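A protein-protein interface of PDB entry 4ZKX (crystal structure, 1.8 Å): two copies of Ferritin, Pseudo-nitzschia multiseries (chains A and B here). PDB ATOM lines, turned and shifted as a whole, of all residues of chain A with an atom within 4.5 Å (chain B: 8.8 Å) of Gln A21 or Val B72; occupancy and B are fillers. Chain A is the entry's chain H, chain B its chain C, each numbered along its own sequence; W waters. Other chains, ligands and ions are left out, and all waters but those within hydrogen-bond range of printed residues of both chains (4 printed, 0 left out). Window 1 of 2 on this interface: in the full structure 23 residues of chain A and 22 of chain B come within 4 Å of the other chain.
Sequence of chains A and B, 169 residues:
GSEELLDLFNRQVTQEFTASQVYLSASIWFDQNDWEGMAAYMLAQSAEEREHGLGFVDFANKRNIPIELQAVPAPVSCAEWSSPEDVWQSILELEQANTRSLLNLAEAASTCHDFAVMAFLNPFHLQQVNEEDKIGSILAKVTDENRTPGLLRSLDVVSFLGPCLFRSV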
ATOM      1  N   PHE A  17      23.413 -27.170   8.383  1.00  0.00           N
ATOM      2  CA  PHE A  17      22.839 -26.380   9.472  1.00  0.00           C
ATOM      3  C   PHE A  17      23.709 -26.441  10.746  1.00  0.00           C
ATOM      4  O   PHE A  17      23.786 -25.471  11.480  1.00  0.00           O
ATOM      5  CB  PHE A  17      21.408 -26.821   9.748  1.00  0.00           C
ATOM      6  CG  PHE A  17      20.419 -26.530   8.642  1.00  0.00           C
ATOM      7  CD1 PHE A  17      20.638 -25.556   7.681  1.00  0.00           C
ATOM      8  CD2 PHE A  17      19.215 -27.200   8.635  1.00  0.00           C
ATOM      9  CE1 PHE A  17      19.660 -25.256   6.748  1.00  0.00           C
ATOM     10  CE2 PHE A  17      18.271 -26.949   7.661  1.00  0.00           C
ATOM     11  CZ  PHE A  17      18.495 -25.962   6.706  1.00  0.00           C
ATOM     12  N   THR A  18      24.370 -27.575  10.973  1.00  0.00           N
ATOM     13  CA  THR A  18      25.321 -27.748  12.064  1.00  0.00           C
ATOM     14  C   THR A  18      26.482 -26.747  11.912  1.00  0.00           C
ATOM     15  O   THR A  18      26.821 -26.018  12.863  1.00  0.00           O
ATOM     16  CB  THR A  18      25.848 -29.195  12.145  1.00  0.00           C
ATOM     17  OG1 THR A  18      24.736 -30.083  12.432  1.00  0.00           O
ATOM     18  CG2 THR A  18      26.901 -29.356  13.194  1.00  0.00           C
ATOM     19  N   ALA A  19      27.031 -26.725  10.718  1.00  0.00           N
ATOM     20  CA  ALA A  19      28.073 -25.711  10.348  1.00  0.00           C
ATOM     21  C   ALA A  19      27.599 -24.257  10.524  1.00  0.00           C
ATOM     22  O   ALA A  19      28.326 -23.439  11.105  1.00  0.00           O
ATOM     23  CB  ALA A  19      28.552 -25.938   8.917  1.00  0.00           C
ATOM     24  N   SER A  20      26.379 -23.949  10.114  1.00  0.00           N
ATOM     25  CA  SER A  20      25.809 -22.629  10.304  1.00  0.00           C
ATOM     26  C   SER A  20      25.813 -22.223  11.751  1.00  0.00           C
ATOM     27  O   SER A  20      26.201 -21.135  12.141  1.00  0.00           O
ATOM     28  CB  SER A  20      24.423 -22.555   9.654  1.00  0.00           C
ATOM     29  OG  SER A  20      23.827 -21.292   9.956  1.00  0.00           O
ATOM     30  N   GLN A  21      25.440 -23.158  12.634  1.00  0.00           N
ATOM     31  CA  GLN A  21      25.447 -22.872  14.068  1.00  0.00           C
ATOM     32  C   GLN A  21      26.830 -22.758  14.662  1.00  0.00           C
ATOM     33  O   GLN A  21      27.051 -21.932  15.541  1.00  0.00           O
ATOM     34  CB  GLN A  21      24.602 -23.976  14.774  1.00  0.00           C
ATOM     35  CG  GLN A  21      23.109 -23.889  14.511  1.00  0.00           C
ATOM     36  CD  GLN A  21      22.516 -22.654  15.180  1.00  0.00           C
ATOM     37  OE1 GLN A  21      22.353 -21.618  14.500  1.00  0.00           O
ATOM     38  NE2 GLN A  21      22.276 -22.708  16.495  1.00  0.00           N
ATOM     39  N   VAL A  22      27.777 -23.541  14.163  1.00  0.00           N
ATOM     40  CA  VAL A  22      29.164 -23.407  14.664  1.00  0.00           C
ATOM     41  C   VAL A  22      29.750 -22.027  14.234  1.00  0.00           C
ATOM     42  O   VAL A  22      30.363 -21.360  15.015  1.00  0.00           O
ATOM     43  CB  VAL A  22      30.096 -24.517  14.138  1.00  0.00           C
ATOM     44  CG1 VAL A  22      31.547 -24.257  14.552  1.00  0.00           C
ATOM     45  CG2 VAL A  22      29.611 -25.874  14.695  1.00  0.00           C
ATOM     46  N   TYR A  23      29.436 -21.591  13.025  1.00  0.00           N
ATOM     47  CA  TYR A  23      29.830 -20.230  12.626  1.00  0.00           C
ATOM     48  C   TYR A  23      29.193 -19.192  13.505  1.00  0.00           C
ATOM     49  O   TYR A  23      29.870 -18.255  13.888  1.00  0.00           O
ATOM     50  CB  TYR A  23      29.530 -19.996  11.144  1.00  0.00           C
ATOM     51  CG  TYR A  23      30.641 -20.432  10.181  1.00  0.00           C
ATOM     52  CD1 TYR A  23      31.774 -19.663   9.997  1.00  0.00           C
ATOM     53  CD2 TYR A  23      30.526 -21.584   9.378  1.00  0.00           C
ATOM     54  CE1 TYR A  23      32.782 -20.062   9.079  1.00  0.00           C
ATOM     55  CE2 TYR A  23      31.482 -21.939   8.430  1.00  0.00           C
ATOM     56  CZ  TYR A  23      32.626 -21.123   8.286  1.00  0.00           C
ATOM     57  OH  TYR A  23      33.620 -21.433   7.415  1.00  0.00           O
ATOM     58  N   LEU A  24      27.905 -19.323  13.833  1.00  0.00           N
ATOM     59  CA  LEU A  24      27.236 -18.444  14.712  1.00  0.00           C
ATOM     60  C   LEU A  24      27.942 -18.419  16.082  1.00  0.00           C
ATOM     61  O   LEU A  24      28.164 -17.359  16.670  1.00  0.00           O
ATOM     62  CB  LEU A  24      25.753 -18.719  14.769  1.00  0.00           C
ATOM     63  CG  LEU A  24      24.944 -17.814  15.721  1.00  0.00           C
ATOM     64  CD1 LEU A  24      25.094 -16.372  15.246  1.00  0.00           C
ATOM     65  CD2 LEU A  24      23.472 -18.250  15.767  1.00  0.00           C
ATOM     66  N   SER A  25      28.281 -19.614  16.589  1.00  0.00           N
ATOM     67  CA  SER A  25      29.008 -19.707  17.830  1.00  0.00           C
ATOM     68  C   SER A  25      30.308 -18.882  17.770  1.00  0.00           C
ATOM     69  O   SER A  25      30.596 -18.128  18.722  1.00  0.00           O
ATOM     70  CB  SER A  25      29.276 -21.180  18.214  1.00  0.00           C
ATOM     71  OG  SER A  25      29.958 -21.270  19.452  1.00  0.00           O
ATOM     72  N   ALA A  71      17.522 -32.722  14.769  1.00  0.00           N
ATOM     73  CA  ALA A  71      18.137 -31.768  15.732  1.00  0.00           C
ATOM     74  C   ALA A  71      19.411 -31.182  15.164  1.00  0.00           C
ATOM     75  O   ALA A  71      20.200 -31.891  14.508  1.00  0.00           O
ATOM     76  CB  ALA A  71      18.434 -32.397  17.087  1.00  0.00           C
ATOM     77  N   VAL A  72      19.573 -29.889  15.363  1.00  0.00           N
ATOM     78  CA  VAL A  72      20.851 -29.206  15.052  1.00  0.00           C
ATOM     79  C   VAL A  72      21.662 -29.158  16.293  1.00  0.00           C
ATOM     80  O   VAL A  72      21.336 -28.479  17.259  1.00  0.00           O
ATOM     81  CB  VAL A  72      20.653 -27.804  14.434  1.00  0.00           C
ATOM     82  CG1 VAL A  72      21.995 -27.261  13.938  1.00  0.00           C
ATOM     83  CG2 VAL A  72      19.711 -27.908  13.238  1.00  0.00           C
ATOM     84  N   PRO A  75      26.676 -26.171  19.422  1.00  0.00           N
ATOM     85  CA  PRO A  75      28.120 -26.083  19.185  1.00  0.00           C
ATOM     86  C   PRO A  75      28.846 -26.307  20.527  1.00  0.00           C
ATOM     87  O   PRO A  75      28.409 -25.838  21.586  1.00  0.00           O
ATOM     88  CB  PRO A  75      28.342 -24.609  18.767  1.00  0.00           C
ATOM     89  CG  PRO A  75      27.082 -24.240  18.173  1.00  0.00           C
ATOM     90  CD  PRO A  75      25.985 -24.934  19.014  1.00  0.00           C
ATOM     91  N   VAL B  13      16.520 -16.989  22.497  1.00  0.00           N
ATOM     92  CA  VAL B  13      17.276 -17.256  21.292  1.00  0.00           C
ATOM     93  C   VAL B  13      16.897 -18.633  20.715  1.00  0.00           C
ATOM     94  O   VAL B  13      16.635 -18.790  19.487  1.00  0.00           O
ATOM     95  CB  VAL B  13      18.804 -17.159  21.523  1.00  0.00           C
ATOM     96  CG1 VAL B  13      19.545 -17.642  20.300  1.00  0.00           C
ATOM     97  CG2 VAL B  13      19.225 -15.708  21.886  1.00  0.00           C
ATOM     98  N   THR B  14      16.922 -19.641  21.595  1.00  0.00           N
ATOM     99  CA  THR B  14      16.567 -20.996  21.216  1.00  0.00           C
ATOM    100  C   THR B  14      15.147 -21.036  20.632  1.00  0.00           C
ATOM    101  O   THR B  14      14.965 -21.672  19.614  1.00  0.00           O
ATOM    102  CB  THR B  14      16.730 -21.962  22.433  1.00  0.00           C
ATOM    103  OG1 THR B  14      18.023 -21.746  22.937  1.00  0.00           O
ATOM    104  CG2 THR B  14      16.547 -23.361  21.948  1.00  0.00           C
ATOM    105  N   GLN B  15      14.173 -20.350  21.240  1.00  0.00           N
ATOM    106  CA  GLN B  15      12.855 -20.394  20.797  1.00  0.00           C
ATOM    107  C   GLN B  15      12.745 -19.791  19.369  1.00  0.00           C
ATOM    108  O   GLN B  15      12.017 -20.345  18.558  1.00  0.00           O
ATOM    109  CB  GLN B  15      11.926 -19.620  21.696  1.00  0.00           C
ATOM    110  CG  GLN B  15      10.469 -19.645  21.200  1.00  0.00           C
ATOM    111  CD  GLN B  15       9.825 -21.064  21.183  1.00  0.00           C
ATOM    112  OE1 GLN B  15      10.169 -21.914  22.027  1.00  0.00           O
ATOM    113  NE2 GLN B  15       8.941 -21.339  20.168  1.00  0.00           N
ATOM    114  N   GLU B  16      13.477 -18.728  19.109  1.00  0.00           N
ATOM    115  CA  GLU B  16      13.448 -18.142  17.773  1.00  0.00           C
ATOM    116  C   GLU B  16      13.976 -19.138  16.734  1.00  0.00           C
ATOM    117  O   GLU B  16      13.392 -19.323  15.660  1.00  0.00           O
ATOM    118  CB  GLU B  16      14.218 -16.821  17.704  1.00  0.00           C
ATOM    119  CG  GLU B  16      13.748 -15.682  18.580  1.00  0.00           C
ATOM    120  CD  GLU B  16      12.381 -15.138  18.258  1.00  0.00           C
ATOM    121  OE1 GLU B  16      11.875 -15.269  17.127  1.00  0.00           O
ATOM    122  OE2 GLU B  16      11.746 -14.720  19.235  1.00  0.00           O
ATOM    123  N   PHE B  17      15.084 -19.796  17.015  1.00  0.00           N
ATOM    124  CA  PHE B  17      15.658 -20.741  16.054  1.00  0.00           C
ATOM    125  C   PHE B  17      14.790 -22.000  15.925  1.00  0.00           C
ATOM    126  O   PHE B  17      14.681 -22.542  14.866  1.00  0.00           O
ATOM    127  CB  PHE B  17      17.075 -21.089  16.484  1.00  0.00           C
ATOM    128  CG  PHE B  17      18.067 -19.919  16.387  1.00  0.00           C
ATOM    129  CD1 PHE B  17      17.854 -18.832  15.614  1.00  0.00           C
ATOM    130  CD2 PHE B  17      19.249 -19.952  17.115  1.00  0.00           C
ATOM    131  CE1 PHE B  17      18.788 -17.775  15.529  1.00  0.00           C
ATOM    132  CE2 PHE B  17      20.154 -18.935  17.047  1.00  0.00           C
ATOM    133  CZ  PHE B  17      19.953 -17.841  16.244  1.00  0.00           C
ATOM    134  N   THR B  18      14.120 -22.415  17.024  1.00  0.00           N
ATOM    135  CA  THR B  18      13.200 -23.550  17.008  1.00  0.00           C
ATOM    136  C   THR B  18      12.067 -23.256  16.056  1.00  0.00           C
ATOM    137  O   THR B  18      11.749 -24.062  15.183  1.00  0.00           O
ATOM    138  CB  THR B  18      12.714 -23.889  18.469  1.00  0.00           C
ATOM    139  OG1 THR B  18      13.876 -24.265  19.269  1.00  0.00           O
ATOM    140  CG2 THR B  18      11.779 -25.064  18.521  1.00  0.00           C
ATOM    141  N   ALA B  19      11.540 -22.060  16.166  1.00  0.00           N
ATOM    142  CA  ALA B  19      10.411 -21.609  15.342  1.00  0.00           C
ATOM    143  C   ALA B  19      10.855 -21.460  13.890  1.00  0.00           C
ATOM    144  O   ALA B  19      10.149 -21.877  12.971  1.00  0.00           O
ATOM    145  CB  ALA B  19       9.849 -20.335  15.854  1.00  0.00           C
ATOM    146  N   SER B  20      12.045 -20.921  13.641  1.00  0.00           N
ATOM    147  CA  SER B  20      12.583 -20.952  12.247  1.00  0.00           C
ATOM    148  C   SER B  20      12.596 -22.351  11.663  1.00  0.00           C
ATOM    149  O   SER B  20      12.267 -22.579  10.526  1.00  0.00           O
ATOM    150  CB  SER B  20      13.980 -20.301  12.227  1.00  0.00           C
ATOM    151  OG  SER B  20      14.599 -20.423  11.016  1.00  0.00           O
ATOM    152  N   GLN B  21      12.958 -23.356  12.447  1.00  0.00           N
ATOM    153  CA  GLN B  21      13.002 -24.713  11.926  1.00  0.00           C
ATOM    154  C   GLN B  21      11.650 -25.271  11.689  1.00  0.00           C
ATOM    155  O   GLN B  21      11.473 -26.074  10.749  1.00  0.00           O
ATOM    156  CB  GLN B  21      13.765 -25.711  12.860  1.00  0.00           C
ATOM    157  CG  GLN B  21      15.225 -25.527  12.882  1.00  0.00           C
ATOM    158  CD  GLN B  21      15.825 -25.997  11.559  1.00  0.00           C
ATOM    159  OE1 GLN B  21      15.982 -25.200  10.644  1.00  0.00           O
ATOM    160  NE2 GLN B  21      16.277 -27.291  11.527  1.00  0.00           N
ATOM    161  N   VAL B  22      10.705 -24.958  12.587  1.00  0.00           N
ATOM    162  CA  VAL B  22       9.305 -25.397  12.426  1.00  0.00           C
ATOM    163  C   VAL B  22       8.718 -24.788  11.128  1.00  0.00           C
ATOM    164  O   VAL B  22       8.157 -25.465  10.314  1.00  0.00           O
ATOM    165  CB  VAL B  22       8.383 -25.060  13.612  1.00  0.00           C
ATOM    166  CG1 VAL B  22       6.953 -25.493  13.301  1.00  0.00           C
ATOM    167  CG2 VAL B  22       8.834 -25.865  14.859  1.00  0.00           C
ATOM    168  N   ARG B  50      14.706 -16.587  12.175  1.00  0.00           N
ATOM    169  CA  ARG B  50      16.111 -16.686  12.426  1.00  0.00           C
ATOM    170  C   ARG B  50      16.684 -15.283  12.623  1.00  0.00           C
ATOM    171  O   ARG B  50      17.469 -15.069  13.506  1.00  0.00           O
ATOM    172  CB  ARG B  50      16.818 -17.426  11.303  1.00  0.00           C
ATOM    173  CG  ARG B  50      18.323 -17.417  11.449  1.00  0.00           C
ATOM    174  CD  ARG B  50      18.970 -18.493  10.575  1.00  0.00           C
ATOM    175  NE  ARG B  50      20.429 -18.512  10.770  1.00  0.00           N
ATOM    176  CZ  ARG B  50      21.226 -17.583  10.242  1.00  0.00           C
ATOM    177  NH1 ARG B  50      20.726 -16.663   9.481  1.00  0.00           N
ATOM    178  NH2 ARG B  50      22.501 -17.565  10.513  1.00  0.00           N
ATOM    179  N   LEU B  54      18.867 -13.738  15.803  1.00  0.00           N
ATOM    180  CA  LEU B  54      20.111 -13.035  15.637  1.00  0.00           C
ATOM    181  C   LEU B  54      20.071 -11.655  16.329  1.00  0.00           C
ATOM    182  O   LEU B  54      21.046 -11.226  16.899  1.00  0.00           O
ATOM    183  CB  LEU B  54      20.480 -12.937  14.189  1.00  0.00           C
ATOM    184  CG  LEU B  54      20.792 -14.234  13.400  1.00  0.00           C
ATOM    185  CD1 LEU B  54      21.053 -13.916  11.946  1.00  0.00           C
ATOM    186  CD2 LEU B  54      21.979 -14.970  14.012  1.00  0.00           C
ATOM    187  N   VAL B  57      20.571 -12.292  19.946  1.00  0.00           N
ATOM    188  CA  VAL B  57      21.998 -12.558  20.199  1.00  0.00           C
ATOM    189  C   VAL B  57      22.841 -11.274  20.215  1.00  0.00           C
ATOM    190  O   VAL B  57      23.670 -11.059  21.111  1.00  0.00           O
ATOM    191  CB  VAL B  57      22.543 -13.511  19.151  1.00  0.00           C
ATOM    192  CG1 VAL B  57      24.051 -13.556  19.237  1.00  0.00           C
ATOM    193  CG2 VAL B  57      21.923 -14.886  19.249  1.00  0.00           C
ATOM    194  N   ILE B  67      25.512 -15.756  26.251  1.00  0.00           N
ATOM    195  CA  ILE B  67      24.653 -16.557  25.399  1.00  0.00           C
ATOM    196  C   ILE B  67      25.445 -17.790  25.234  1.00  0.00           C
ATOM    197  O   ILE B  67      26.653 -17.681  25.004  1.00  0.00           O
ATOM    198  CB  ILE B  67      24.460 -15.939  23.963  1.00  0.00           C
ATOM    199  CG1 ILE B  67      23.610 -14.721  24.019  1.00  0.00           C
ATOM    200  CG2 ILE B  67      23.831 -16.988  22.952  1.00  0.00           C
ATOM    201  CD1 ILE B  67      22.239 -14.965  24.626  1.00  0.00           C
ATOM    202  N   GLU B  68      24.796 -18.931  25.351  1.00  0.00           N
ATOM    203  CA  GLU B  68      25.400 -20.131  24.841  1.00  0.00           C
ATOM    204  C   GLU B  68      24.370 -20.886  24.002  1.00  0.00           C
ATOM    205  O   GLU B  68      23.271 -21.228  24.496  1.00  0.00           O
ATOM    206  CB  GLU B  68      25.960 -20.984  25.981  1.00  0.00           C
ATOM    207  CG  GLU B  68      27.233 -20.306  26.481  1.00  0.00           C
ATOM    208  CD  GLU B  68      28.155 -21.179  27.294  1.00  0.00           C
ATOM    209  OE1 GLU B  68      27.615 -22.113  27.925  1.00  0.00           O
ATOM    210  OE2 GLU B  68      29.392 -20.873  27.304  1.00  0.00           O
ATOM    211  N   LEU B  69      24.765 -21.119  22.739  1.00  0.00           N
ATOM    212  CA  LEU B  69      23.846 -21.722  21.823  1.00  0.00           C
ATOM    213  C   LEU B  69      23.508 -23.155  22.268  1.00  0.00           C
ATOM    214  O   LEU B  69      24.397 -24.002  22.568  1.00  0.00           O
ATOM    215  CB  LEU B  69      24.400 -21.707  20.433  1.00  0.00           C
ATOM    216  CG  LEU B  69      24.630 -20.323  19.813  1.00  0.00           C
ATOM    217  CD1 LEU B  69      25.221 -20.426  18.443  1.00  0.00           C
ATOM    218  CD2 LEU B  69      23.230 -19.603  19.751  1.00  0.00           C
ATOM    219  N   GLN B  70      22.233 -23.415  22.279  1.00  0.00           N
ATOM    220  CA  GLN B  70      21.626 -24.694  22.590  1.00  0.00           C
ATOM    221  C   GLN B  70      21.398 -25.454  21.283  1.00  0.00           C
ATOM    222  O   GLN B  70      21.368 -24.861  20.153  1.00  0.00           O
ATOM    223  CB  GLN B  70      20.349 -24.485  23.407  1.00  0.00           C
ATOM    224  CG  GLN B  70      20.524 -23.714  24.714  1.00  0.00           C
ATOM    225  CD  GLN B  70      21.545 -24.388  25.610  1.00  0.00           C
ATOM    226  OE1 GLN B  70      21.317 -25.511  26.084  1.00  0.00           O
ATOM    227  NE2 GLN B  70      22.680 -23.707  25.856  1.00  0.00           N
ATOM    228  N   ALA B  71      21.179 -26.764  21.399  1.00  0.00           N
ATOM    229  CA  ALA B  71      20.720 -27.498  20.278  1.00  0.00           C
ATOM    230  C   ALA B  71      19.359 -26.889  19.821  1.00  0.00           C
ATOM    231  O   ALA B  71      18.584 -26.354  20.613  1.00  0.00           O
ATOM    232  CB  ALA B  71      20.543 -28.997  20.592  1.00  0.00           C
ATOM    233  N   VAL B  72      19.192 -26.916  18.513  1.00  0.00           N
ATOM    234  CA  VAL B  72      17.891 -26.601  17.894  1.00  0.00           C
ATOM    235  C   VAL B  72      17.081 -27.865  17.700  1.00  0.00           C
ATOM    236  O   VAL B  72      17.352 -28.719  16.853  1.00  0.00           O
ATOM    237  CB  VAL B  72      17.981 -25.820  16.585  1.00  0.00           C
ATOM    238  CG1 VAL B  72      16.610 -25.297  16.218  1.00  0.00           C
ATOM    239  CG2 VAL B  72      18.934 -24.661  16.729  1.00  0.00           C
ATOM    240  N   PRO B  73      16.025 -27.988  18.502  1.00  0.00           N
ATOM    241  CA  PRO B  73      15.331 -29.265  18.404  1.00  0.00           C
ATOM    242  C   PRO B  73      14.714 -29.525  17.057  1.00  0.00           C
ATOM    243  O   PRO B  73      14.224 -28.597  16.420  1.00  0.00           O
ATOM    244  CB  PRO B  73      14.205 -29.116  19.429  1.00  0.00           C
ATOM    245  CG  PRO B  73      14.708 -28.119  20.469  1.00  0.00           C
ATOM    246  CD  PRO B  73      15.480 -27.133  19.581  1.00  0.00           C
ATOM    247  N   ALA B  74      14.627 -30.787  16.659  1.00  0.00           N
ATOM    248  CA  ALA B  74      13.905 -31.227  15.474  1.00  0.00           C
ATOM    249  C   ALA B  74      12.456 -30.839  15.582  1.00  0.00           C
ATOM    250  O   ALA B  74      11.796 -31.037  16.648  1.00  0.00           O
ATOM    251  CB  ALA B  74      14.041 -32.729  15.267  1.00  0.00           C
ATOM    252  N   PRO B  75      11.884 -30.344  14.454  1.00  0.00           N
ATOM    253  CA  PRO B  75      10.439 -30.155  14.434  1.00  0.00           C
ATOM    254  C   PRO B  75       9.753 -31.515  14.553  1.00  0.00           C
ATOM    255  O   PRO B  75      10.233 -32.504  14.002  1.00  0.00           O
ATOM    256  CB  PRO B  75      10.142 -29.557  13.062  1.00  0.00           C
ATOM    257  CG  PRO B  75      11.447 -28.930  12.658  1.00  0.00           C
ATOM    258  CD  PRO B  75      12.584 -29.706  13.317  1.00  0.00           C
HETATM  259  O   HOH W   1      27.263 -23.534  22.337  1.00  0.00           O
HETATM  260  O   HOH W   2      22.538 -25.439  17.652  1.00  0.00           O
HETATM  261  O   HOH W   3      20.752 -22.298  19.125  1.00  0.00           O
HETATM  262  O   HOH W   4      22.630 -20.078  12.084  1.00  0.00           O
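Of the 22 printed residues of chain B, 8 touch a printed residue of chain A. Printed residues of chain B that touch a printed residue of chain A: Phe B17, Gln B21, Arg B50, Leu B54, Leu B69, Ala B71, Val B72 and Ala B74. Hydrophobic or aromatic side chains of chain B within 4 Å of the printed part of chain A: Phe B17, Leu B54, Leu B69, Ala B71, Val B72 and Ala B74. Of the 12 printed residues of chain A, 7 touch a printed residue of chain B. Hydrophobic or aromatic side chains of chain A that line the printed part of chain B: Leu A24, Ala A71, Val A72 and Pro A75. Among the printed residues, no Asp or Glu carboxylate lies within 4 Å of a Lys or Arg side-chain nitrogen of the other chain.
Of the printed residues of chain B, Ser A20 touches Arg B50 (3.99 Å). Of chain B, only Leu B69 (3.7 Å) and Val B72 (3.9 Å) come within 4 Å of Gln A21. Val A22 touches none of the printed residues of chain B. Of the printed residues of chain B, Ala A71 touches Val B72 and Ala B74. Of chain B, only Gln B21, Ala B71 and Val B72 come within 4 Å of Val A72. Ala B19 touches none of the printed residues of chain A. Printed residues of chain A within 4 Å of Leu B54: Leu A24. Of the printed residues of chain A, Leu B69 touches Gln A21, Leu A24, Ser A25 and Pro A75. Val B72 touches just these residues of chain A: Gln A21 (3.9 Å), Ala A71 (3.3 Å) and Val A72 (2.9 Å). Of the printed residues of chain A, Ala B74 touches Ala A71 (3.5 Å). The nearest residue of chain B that does not touch Gln A21 is Phe B17 (4.1 Å). The nearest printed residue of chain A that does not touch Val B72 is Pro A75 (7.1 Å). The nearest printed residue of chain B that does not touch Ala A71 is Pro B73 (4.3 Å).
Among the printed residues, pairs that only touch across the chains: Ser A20 with Arg B50, Gln A21 with Leu B69, Gln A21 with Val B72, Leu A24 with Phe B17, Leu A24 with Leu B54, Leu A24 with Leu B69, Ser A25 with Leu B69, Ala A71 with Val B72, Ala A71 with Ala B74, Val A72 with Gln B21, Val A72 with Ala B71 and Pro A75 with Leu B69.
Gln A21 touches Val B72, and with the chains exchanged Val A72 touches Gln B21. Ala A71 touches Val B72, and with the chains exchanged Val A72 touches Ala B71. Val A72 touches its own counterpart, Val B72.
Water W1 lies within hydrogen-bond range of O of Pro A75 and O of Leu B69. Water W4 lies within hydrogen-bond range of OG of Ser A20 (2.7 Å), OE1 of Gln A21 (2.9 Å) and NH2 of Arg B50 (3.0 Å). Water W2 lies within hydrogen-bond range of O of Gln B70 (2.8 Å), NE2 of Gln A21 (3.0 Å) and O of Val A72 (3.3 Å). Water W3 bridges the backbone carbonyl oxygen of Gln B70 (2.8 Å) and the side-chain amide nitrogen of Gln A21 (3.1 Å).
The backbone NH (N) of Val A72 is in hydrogen-bond range of the backbone carbonyl oxygen (O) of Val B72 (2.9 Å).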
